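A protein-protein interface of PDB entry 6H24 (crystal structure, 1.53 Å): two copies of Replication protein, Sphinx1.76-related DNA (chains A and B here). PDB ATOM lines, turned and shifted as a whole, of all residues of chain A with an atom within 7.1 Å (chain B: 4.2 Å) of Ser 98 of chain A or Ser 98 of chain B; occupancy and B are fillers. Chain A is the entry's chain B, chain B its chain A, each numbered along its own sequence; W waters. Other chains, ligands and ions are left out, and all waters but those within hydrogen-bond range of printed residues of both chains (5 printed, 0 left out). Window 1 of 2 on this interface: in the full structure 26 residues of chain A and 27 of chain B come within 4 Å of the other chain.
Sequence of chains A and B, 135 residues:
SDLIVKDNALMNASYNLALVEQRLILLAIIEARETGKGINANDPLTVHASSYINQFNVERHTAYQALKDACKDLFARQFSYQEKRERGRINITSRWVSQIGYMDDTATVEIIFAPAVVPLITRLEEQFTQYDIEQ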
ATOM      1  N   ALA A  41      21.089  16.958  10.757  1.00  0.00           N
ATOM      2  CA  ALA A  41      21.277  15.514  10.721  1.00  0.00           C
ATOM      3  C   ALA A  41      21.381  14.956   9.307  1.00  0.00           C
ATOM      4  O   ALA A  41      21.465  13.733   9.149  1.00  0.00           O
ATOM      5  CB  ALA A  41      20.131  14.819  11.464  1.00  0.00           C
ATOM      6  N   ASN A  42      21.388  15.811   8.287  1.00  0.00           N
ATOM      7  CA  ASN A  42      21.460  15.374   6.900  1.00  0.00           C
ATOM      8  C   ASN A  42      22.772  15.711   6.207  1.00  0.00           C
ATOM      9  O   ASN A  42      23.207  14.951   5.342  1.00  0.00           O
ATOM     10  CB  ASN A  42      20.322  16.004   6.074  1.00  0.00           C
ATOM     11  CG  ASN A  42      19.100  15.121   5.998  1.00  0.00           C
ATOM     12  OD1 ASN A  42      19.059  14.167   5.222  1.00  0.00           O
ATOM     13  ND2 ASN A  42      18.085  15.445   6.790  1.00  0.00           N
ATOM     14  N   PHE A  75      32.722   7.125  15.273  1.00  0.00           N
ATOM     15  CA  PHE A  75      31.655   6.358  14.628  1.00  0.00           C
ATOM     16  C   PHE A  75      31.293   5.105  15.421  1.00  0.00           C
ATOM     17  O   PHE A  75      30.135   4.670  15.411  1.00  0.00           O
ATOM     18  CB  PHE A  75      32.139   6.008  13.213  1.00  0.00           C
ATOM     19  CG  PHE A  75      31.127   5.306  12.350  1.00  0.00           C
ATOM     20  CD1 PHE A  75      30.178   6.035  11.641  1.00  0.00           C
ATOM     21  CD2 PHE A  75      31.168   3.931  12.178  1.00  0.00           C
ATOM     22  CE1 PHE A  75      29.266   5.399  10.827  1.00  0.00           C
ATOM     23  CE2 PHE A  75      30.263   3.288  11.364  1.00  0.00           C
ATOM     24  CZ  PHE A  75      29.303   4.024  10.680  1.00  0.00           C
ATOM     25  N   THR A  93      19.037   4.708  22.528  1.00  0.00           N
ATOM     26  CA  THR A  93      20.465   4.636  22.262  1.00  0.00           C
ATOM     27  C   THR A  93      20.757   5.399  20.975  1.00  0.00           C
ATOM     28  O   THR A  93      20.071   5.204  19.967  1.00  0.00           O
ATOM     29  CB  THR A  93      20.938   3.189  22.125  1.00  0.00           C
ATOM     30  OG1 THR A  93      20.559   2.446  23.291  1.00  0.00           O
ATOM     31  CG2 THR A  93      22.453   3.151  21.969  1.00  0.00           C
ATOM     32  N   SER A  94      21.778   6.259  21.012  1.00  0.00           N
ATOM     33  CA  SER A  94      22.120   7.103  19.881  1.00  0.00           C
ATOM     34  C   SER A  94      23.597   6.961  19.553  1.00  0.00           C
ATOM     35  O   SER A  94      24.437   6.730  20.435  1.00  0.00           O
ATOM     36  CB  SER A  94      21.815   8.582  20.167  1.00  0.00           C
ATOM     37  OG  SER A  94      22.163   9.402  19.070  1.00  0.00           O
ATOM     38  N   ARG A  95      23.896   7.150  18.272  1.00  0.00           N
ATOM     39  CA  ARG A  95      25.246   7.390  17.811  1.00  0.00           C
ATOM     40  C   ARG A  95      25.622   8.848  18.043  1.00  0.00           C
ATOM     41  O   ARG A  95      24.773   9.698  18.319  1.00  0.00           O
ATOM     42  CB  ARG A  95      25.369   7.062  16.321  1.00  0.00           C
ATOM     43  CG  ARG A  95      25.167   5.595  15.995  1.00  0.00           C
ATOM     44  CD  ARG A  95      26.173   4.718  16.712  1.00  0.00           C
ATOM     45  NE  ARG A  95      26.026   3.321  16.342  1.00  0.00           N
ATOM     46  CZ  ARG A  95      26.766   2.343  16.846  1.00  0.00           C
ATOM     47  NH1 ARG A  95      27.715   2.635  17.732  1.00  0.00           N
ATOM     48  NH2 ARG A  95      26.585   1.092  16.460  1.00  0.00           N
ATOM     49  N   TRP A  96      26.927   9.117  17.965  1.00  0.00           N
ATOM     50  CA  TRP A  96      27.395  10.493  17.859  1.00  0.00           C
ATOM     51  C   TRP A  96      27.279  11.008  16.426  1.00  0.00           C
ATOM     52  O   TRP A  96      26.878  12.158  16.199  1.00  0.00           O
ATOM     53  CB  TRP A  96      28.847  10.616  18.306  1.00  0.00           C
ATOM     54  CG  TRP A  96      29.110  10.542  19.781  1.00  0.00           C
ATOM     55  CD1 TRP A  96      29.169   9.427  20.556  1.00  0.00           C
ATOM     56  CD2 TRP A  96      29.339  11.654  20.651  1.00  0.00           C
ATOM     57  NE1 TRP A  96      29.440   9.774  21.864  1.00  0.00           N
ATOM     58  CE2 TRP A  96      29.551  11.140  21.942  1.00  0.00           C
ATOM     59  CE3 TRP A  96      29.401  13.036  20.454  1.00  0.00           C
ATOM     60  CZ2 TRP A  96      29.803  11.964  23.039  1.00  0.00           C
ATOM     61  CZ3 TRP A  96      29.661  13.852  21.545  1.00  0.00           C
ATOM     62  CH2 TRP A  96      29.862  13.314  22.815  1.00  0.00           C
ATOM     63  N   VAL A  97      27.668  10.180  15.454  1.00  0.00           N
ATOM     64  CA  VAL A  97      27.640  10.516  14.037  1.00  0.00           C
ATOM     65  C   VAL A  97      26.979   9.351  13.308  1.00  0.00           C
ATOM     66  O   VAL A  97      27.197   8.186  13.660  1.00  0.00           O
ATOM     67  CB  VAL A  97      29.059  10.781  13.481  1.00  0.00           C
ATOM     68  CG1 VAL A  97      29.668  12.048  14.095  1.00  0.00           C
ATOM     69  CG2 VAL A  97      29.984   9.576  13.720  1.00  0.00           C
ATOM     70  N   SER A  98      26.159   9.661  12.302  1.00  0.00           N
ATOM     71  CA  SER A  98      25.506   8.632  11.503  1.00  0.00           C
ATOM     72  C   SER A  98      26.348   8.196  10.312  1.00  0.00           C
ATOM     73  O   SER A  98      26.087   7.132   9.734  1.00  0.00           O
ATOM     74  CB  SER A  98      24.163   9.167  10.994  1.00  0.00           C
ATOM     75  OG  SER A  98      24.388  10.366  10.292  1.00  0.00           O
ATOM     76  N   GLN A  99      27.360   8.981   9.955  1.00  0.00           N
ATOM     77  CA  GLN A  99      28.101   8.809   8.721  1.00  0.00           C
ATOM     78  C   GLN A  99      29.453   9.485   8.880  1.00  0.00           C
ATOM     79  O   GLN A  99      29.552  10.534   9.523  1.00  0.00           O
ATOM     80  CB  GLN A  99      27.334   9.419   7.540  1.00  0.00           C
ATOM     81  CG  GLN A  99      27.958   9.190   6.189  1.00  0.00           C
ATOM     82  CD  GLN A  99      27.194   9.893   5.089  1.00  0.00           C
ATOM     83  OE1 GLN A  99      27.764  10.700   4.353  1.00  0.00           O
ATOM     84  NE2 GLN A  99      25.909   9.588   4.963  1.00  0.00           N
ATOM     85  N   ILE A 100      30.484   8.867   8.302  1.00  0.00           N
ATOM     86  CA  ILE A 100      31.819   9.443   8.229  1.00  0.00           C
ATOM     87  C   ILE A 100      32.327   9.286   6.801  1.00  0.00           C
ATOM     88  O   ILE A 100      31.782   8.525   5.998  1.00  0.00           O
ATOM     89  CB  ILE A 100      32.803   8.800   9.228  1.00  0.00           C
ATOM     90  CG1 ILE A 100      32.930   7.292   8.994  1.00  0.00           C
ATOM     91  CG2 ILE A 100      32.357   9.049  10.663  1.00  0.00           C
ATOM     92  CD1 ILE A 100      34.021   6.611   9.827  1.00  0.00           C
ATOM     93  N   ILE A 111      31.919  14.327   8.662  1.00  0.00           N
ATOM     94  CA  ILE A 111      31.010  13.674   9.596  1.00  0.00           C
ATOM     95  C   ILE A 111      29.611  14.243   9.403  1.00  0.00           C
ATOM     96  O   ILE A 111      29.442  15.395   8.995  1.00  0.00           O
ATOM     97  CB  ILE A 111      31.469  13.830  11.062  1.00  0.00           C
ATOM     98  CG1 ILE A 111      31.460  15.294  11.507  1.00  0.00           C
ATOM     99  CG2 ILE A 111      32.864  13.253  11.226  1.00  0.00           C
ATOM    100  CD1 ILE A 111      31.730  15.483  13.004  1.00  0.00           C
ATOM    101  N   ILE A 112      28.605  13.425   9.708  1.00  0.00           N
ATOM    102  CA  ILE A 112      27.235  13.898   9.898  1.00  0.00           C
ATOM    103  C   ILE A 112      26.857  13.565  11.342  1.00  0.00           C
ATOM    104  O   ILE A 112      26.903  12.393  11.751  1.00  0.00           O
ATOM    105  CB  ILE A 112      26.228  13.265   8.933  1.00  0.00           C
ATOM    106  CG1 ILE A 112      26.651  13.393   7.470  1.00  0.00           C
ATOM    107  CG2 ILE A 112      24.857  13.937   9.103  1.00  0.00           C
ATOM    108  CD1 ILE A 112      25.632  12.796   6.476  1.00  0.00           C
ATOM    109  N   PHE A 113      26.442  14.574  12.097  1.00  0.00           N
ATOM    110  CA  PHE A 113      26.022  14.347  13.469  1.00  0.00           C
ATOM    111  C   PHE A 113      24.684  13.620  13.503  1.00  0.00           C
ATOM    112  O   PHE A 113      23.798  13.881  12.680  1.00  0.00           O
ATOM    113  CB  PHE A 113      25.890  15.672  14.222  1.00  0.00           C
ATOM    114  CG  PHE A 113      27.197  16.329  14.546  1.00  0.00           C
ATOM    115  CD1 PHE A 113      28.042  15.779  15.493  1.00  0.00           C
ATOM    116  CD2 PHE A 113      27.556  17.522  13.945  1.00  0.00           C
ATOM    117  CE1 PHE A 113      29.234  16.389  15.809  1.00  0.00           C
ATOM    118  CE2 PHE A 113      28.761  18.144  14.264  1.00  0.00           C
ATOM    119  CZ  PHE A 113      29.596  17.568  15.200  1.00  0.00           C
ATOM    120  N   ALA A 114      24.534  12.729  14.477  1.00  0.00           N
ATOM    121  CA  ALA A 114      23.259  12.061  14.708  1.00  0.00           C
ATOM    122  C   ALA A 114      22.223  13.070  15.192  1.00  0.00           C
ATOM    123  O   ALA A 114      22.573  14.075  15.816  1.00  0.00           O
ATOM    124  CB  ALA A 114      23.418  10.954  15.747  1.00  0.00           C
ATOM    125  N   PRO A 115      20.935  12.825  14.931  1.00  0.00           N
ATOM    126  CA  PRO A 115      19.932  13.851  15.265  1.00  0.00           C
ATOM    127  C   PRO A 115      19.816  14.156  16.755  1.00  0.00           C
ATOM    128  O   PRO A 115      19.435  15.282  17.108  1.00  0.00           O
ATOM    129  CB  PRO A 115      18.628  13.280  14.677  1.00  0.00           C
ATOM    130  CG  PRO A 115      18.876  11.856  14.459  1.00  0.00           C
ATOM    131  CD  PRO A 115      20.343  11.676  14.221  1.00  0.00           C
ATOM    132  N   ALA A 116      20.141  13.207  17.645  1.00  0.00           N
ATOM    133  CA  ALA A 116      20.075  13.497  19.077  1.00  0.00           C
ATOM    134  C   ALA A 116      21.159  14.472  19.509  1.00  0.00           C
ATOM    135  O   ALA A 116      20.985  15.182  20.505  1.00  0.00           O
ATOM    136  CB  ALA A 116      20.190  12.208  19.894  1.00  0.00           C
ATOM    137  N   PHE B  75      21.274  -1.618  14.682  1.00  0.00           N
ATOM    138  CA  PHE B  75      22.066  -0.472  15.128  1.00  0.00           C
ATOM    139  C   PHE B  75      23.564  -0.754  15.058  1.00  0.00           C
ATOM    140  O   PHE B  75      24.355   0.166  14.840  1.00  0.00           O
ATOM    141  CB  PHE B  75      21.590  -0.130  16.544  1.00  0.00           C
ATOM    142  CG  PHE B  75      22.239   1.070  17.166  1.00  0.00           C
ATOM    143  CD1 PHE B  75      21.769   2.346  16.925  1.00  0.00           C
ATOM    144  CD2 PHE B  75      23.282   0.905  18.057  1.00  0.00           C
ATOM    145  CE1 PHE B  75      22.346   3.438  17.535  1.00  0.00           C
ATOM    146  CE2 PHE B  75      23.872   2.000  18.670  1.00  0.00           C
ATOM    147  CZ  PHE B  75      23.403   3.268  18.408  1.00  0.00           C
ATOM    148  N   SER B  94      28.549   4.419   6.533  1.00  0.00           N
ATOM    149  CA  SER B  94      27.257   4.847   7.053  1.00  0.00           C
ATOM    150  C   SER B  94      26.659   3.769   7.939  1.00  0.00           C
ATOM    151  O   SER B  94      26.926   2.581   7.760  1.00  0.00           O
ATOM    152  CB  SER B  94      26.252   5.160   5.914  1.00  0.00           C
ATOM    153  OG  SER B  94      24.979   5.547   6.417  1.00  0.00           O
ATOM    154  N   ARG B  95      25.854   4.205   8.905  1.00  0.00           N
ATOM    155  CA  ARG B  95      24.956   3.326   9.627  1.00  0.00           C
ATOM    156  C   ARG B  95      23.682   3.082   8.820  1.00  0.00           C
ATOM    157  O   ARG B  95      23.389   3.785   7.850  1.00  0.00           O
ATOM    158  CB  ARG B  95      24.586   3.931  10.983  1.00  0.00           C
ATOM    159  CG  ARG B  95      25.756   4.091  11.958  1.00  0.00           C
ATOM    160  CD  ARG B  95      26.400   2.765  12.258  1.00  0.00           C
ATOM    161  NE  ARG B  95      27.471   2.891  13.243  1.00  0.00           N
ATOM    162  CZ  ARG B  95      28.198   1.883  13.681  1.00  0.00           C
ATOM    163  NH1 ARG B  95      27.968   0.643  13.260  1.00  0.00           N
ATOM    164  NH2 ARG B  95      29.157   2.102  14.571  1.00  0.00           N
ATOM    165  N   VAL B  97      20.788   2.920  10.863  1.00  0.00           N
ATOM    166  CA  VAL B  97      19.975   3.740  11.750  1.00  0.00           C
ATOM    167  C   VAL B  97      20.909   4.537  12.660  1.00  0.00           C
ATOM    168  O   VAL B  97      21.958   4.038  13.080  1.00  0.00           O
ATOM    169  CB  VAL B  97      18.998   2.874  12.578  1.00  0.00           C
ATOM    170  CG1 VAL B  97      17.913   2.270  11.701  1.00  0.00           C
ATOM    171  CG2 VAL B  97      19.756   1.750  13.305  1.00  0.00           C
ATOM    172  N   SER B  98      20.543   5.787  12.932  1.00  0.00           N
ATOM    173  CA  SER B  98      21.320   6.641  13.817  1.00  0.00           C
ATOM    174  C   SER B  98      20.896   6.525  15.273  1.00  0.00           C
ATOM    175  O   SER B  98      21.655   6.940  16.165  1.00  0.00           O
ATOM    176  CB  SER B  98      21.182   8.103  13.385  1.00  0.00           C
ATOM    177  OG  SER B  98      19.816   8.487  13.353  1.00  0.00           O
ATOM    178  N   GLN B  99      19.709   5.982  15.535  1.00  0.00           N
ATOM    179  CA  GLN B  99      19.094   6.018  16.851  1.00  0.00           C
ATOM    180  C   GLN B  99      18.066   4.908  16.928  1.00  0.00           C
ATOM    181  O   GLN B  99      17.342   4.669  15.958  1.00  0.00           O
ATOM    182  CB  GLN B  99      18.411   7.374  17.098  1.00  0.00           C
ATOM    183  CG  GLN B  99      17.831   7.595  18.494  1.00  0.00           C
ATOM    184  CD  GLN B  99      17.100   8.922  18.616  1.00  0.00           C
ATOM    185  OE1 GLN B  99      15.921   8.972  18.989  1.00  0.00           O
ATOM    186  NE2 GLN B  99      17.786   9.999  18.286  1.00  0.00           N
ATOM    187  N   ILE B 112      15.410   5.791  13.926  1.00  0.00           N
ATOM    188  CA  ILE B 112      15.638   6.834  12.935  1.00  0.00           C
ATOM    189  C   ILE B 112      16.620   6.304  11.901  1.00  0.00           C
ATOM    190  O   ILE B 112      17.716   5.862  12.256  1.00  0.00           O
ATOM    191  CB  ILE B 112      16.179   8.134  13.547  1.00  0.00           C
ATOM    192  CG1 ILE B 112      15.311   8.609  14.715  1.00  0.00           C
ATOM    193  CG2 ILE B 112      16.227   9.213  12.462  1.00  0.00           C
ATOM    194  CD1 ILE B 112      15.784   9.918  15.344  1.00  0.00           C
ATOM    195  N   ALA B 114      19.460   6.454   9.070  1.00  0.00           N
ATOM    196  CA  ALA B 114      20.583   7.306   8.729  1.00  0.00           C
ATOM    197  C   ALA B 114      20.324   8.016   7.403  1.00  0.00           C
ATOM    198  O   ALA B 114      19.608   7.500   6.540  1.00  0.00           O
ATOM    199  CB  ALA B 114      21.860   6.484   8.635  1.00  0.00           C
ATOM    200  N   PRO B 115      20.912   9.198   7.204  1.00  0.00           N
ATOM    201  CA  PRO B 115      20.551   9.970   5.997  1.00  0.00           C
ATOM    202  C   PRO B 115      20.918   9.299   4.685  1.00  0.00           C
ATOM    203  O   PRO B 115      20.230   9.518   3.684  1.00  0.00           O
ATOM    204  CB  PRO B 115      21.294  11.302   6.182  1.00  0.00           C
ATOM    205  CG  PRO B 115      22.335  11.053   7.243  1.00  0.00           C
ATOM    206  CD  PRO B 115      21.805   9.941   8.112  1.00  0.00           C
HETATM  207  O   HOH W   1      20.237  10.384  17.191  1.00  0.00           O
HETATM  208  O   HOH W   2      24.139   8.209   6.601  1.00  0.00           O
HETATM  209  O   HOH W   3      24.059   2.823  14.393  1.00  0.00           O
HETATM  210  O   HOH W   4      27.877   5.511  14.186  1.00  0.00           O
HETATM  211  O   HOH W   5      16.786  12.557  18.229  1.00  0.00           O
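The backbone NH of Arg 95 of chain B lies within hydrogen-bond range of the backbone carbonyl oxygen of Ser 98 of chain A (3.1 Å). The guanidinium group of Arg 95 of chain B is in hydrogen-bond range of the backbone carbonyl oxygen of Phe 75 of chain A (2.9 Å). The backbone carbonyl oxygen (O) of Ser 98 of chain B is in hydrogen-bond range of the backbone NH (N) of Arg 95 of chain A (3.1 Å). NH2 of Arg 95 of chain A lies close to NH2 of Arg 95 of chain B (3.3 Å). The guanidinium group (NH2) of Arg 95 of chain A is in hydrogen-bond range of the backbone carbonyl oxygen (O) of Phe 75 of chain B.
Phe 75 of chain A touches Ser 94 of chain B, and with the chains exchanged Ser 94 of chain A touches Phe 75 of chain B. Phe 75 of chain A touches Arg 95 of chain B, and with the chains exchanged Arg 95 of chain A touches Phe 75 of chain B. Arg 95 of chain A touches Ser 98 of chain B, and with the chains exchanged Ser 98 of chain A touches Arg 95 of chain B. Ser 98 of chain A touches Pro 115 of chain B, and with the chains exchanged Pro 115 of chain A touches Ser 98 of chain B. Of the 19 pairs that touch across the chains among the printed residues, 14 have their exchanged pair printed and touching as well.
Ala 41 of chain A touches Pro 115 of chain B (O to CG, 3.4 Å). OD1 of Asn 42 of chain A touches CB of Pro 115 of chain B, at 3.8 Å. Phe 75 of chain B touches Thr 93 of chain A (CZ to CG2, 3.7 Å). O of Thr 93 of chain A touches CA of Gln 99 of chain B, at 3.4 Å. Ser 94 of chain A touches Ser 98 of chain B (CA to O, 3.7 Å). Ser 94 of chain B touches Ser 98 of chain A. Ser 98 of chain A touches Ser 98 of chain B. OG of Ser 98 of chain A touches CD of Pro 115 of chain B (3.4 Å). Ser 98 of chain B touches Pro 115 of chain A. CG of Pro 115 of chain A touches CD1 of Ile 112 of chain B, at 3.8 Å.
Water W4 lies within hydrogen-bond range of the backbone carbonyl oxygen of Phe 75 of chain A (2.7 Å), the backbone carbonyl oxygen of Val 97 of chain A (2.8 Å) and the guanidinium group of Arg 95 of chain B (2.8 Å). Water W3 lies within hydrogen-bond range of O of Phe 75 of chain B (2.7 Å), O of Val 97 of chain B (2.8 Å) and NE of Arg 95 of chain A (2.8 Å). Water W1 lies within hydrogen-bond range of NE2 of Gln 99 of chain B (2.7 Å), N of Ala 116 of chain A (2.9 Å) and OG of Ser 94 of chain A (2.9 Å). Water W5 bridges the side-chain amide nitrogen (NE2) of Gln 99 of chain B and the backbone NH (N) of Ala 116 of chain A. Water W2 lies within hydrogen-bond range of the side-chain amide nitrogen (NE2) of Gln 99 of chain A (2.8 Å) and the side-chain hydroxyl (OG) of Ser 94 of chain B (2.8 Å).
Ser 98 of chain A touches just these residues of chain B: Ser 94 (3.7 Å), Arg 95 (3.1 Å), Ser 98 (3.97 Å) and Pro 115 (3.4 Å). Ser 98 of chain B touches just these residues of chain A: Ser 94, Arg 95, Ser 98 and Pro 115. Of the printed residues of chain A, Phe 75 of chain B touches Thr 93 (3.7 Å), Ser 94 (3.9 Å) and Arg 95 (2.9 Å). Of the printed residues of chain A, Gln 99 of chain B touches Thr 93 (3.4 Å) and Ala 116 (3.6 Å). Val 97 of chain B touches none of the printed residues of chain A. The nearest printed residue of chain B that does not touch Ser 98 of chain A is Ala 114 of chain B (4.3 Å). The nearest residue of chain A that does not touch Ser 98 of chain B is Ala 114 of chain A (4.3 Å). The nearest printed residue of chain B that does not touch Ile 112 of chain A is Ala 114 of chain B (7.2 Å).
Hydrophobic or aromatic side chains of chain B within 4 Å of the printed part of chain A: Phe 75, Ile 112 and Pro 115. Printed residues of chain A that touch a printed residue of chain B: Ala 41, Asn 42, Phe 75, Thr 93, Ser 94, Arg 95, Ser 98, Ile 112, Pro 115 and Ala 116. Among the printed residues, no Asp or Glu carboxylate lies within 4 Å of a Lys or Arg side-chain nitrogen of the other chain.
The backbone NH of Ile 112 of chain A is in hydrogen-bond range of the backbone carbonyl oxygen of Gln 99 of chain A (3.0 Å). The backbone carbonyl oxygen (O) of Ile 112 of chain B is in hydrogen-bond range of the backbone NH (N) of Ser 98 of chain B (2.9 Å). The backbone carbonyl oxygen of Ile 112 of chain A sits at hydrogen-bond distance from the backbone NH of Ser 98 of chain A (2.9 Å). N of Ile 112 of chain B sits at hydrogen-bond distance from O of Gln 99 of chain B.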
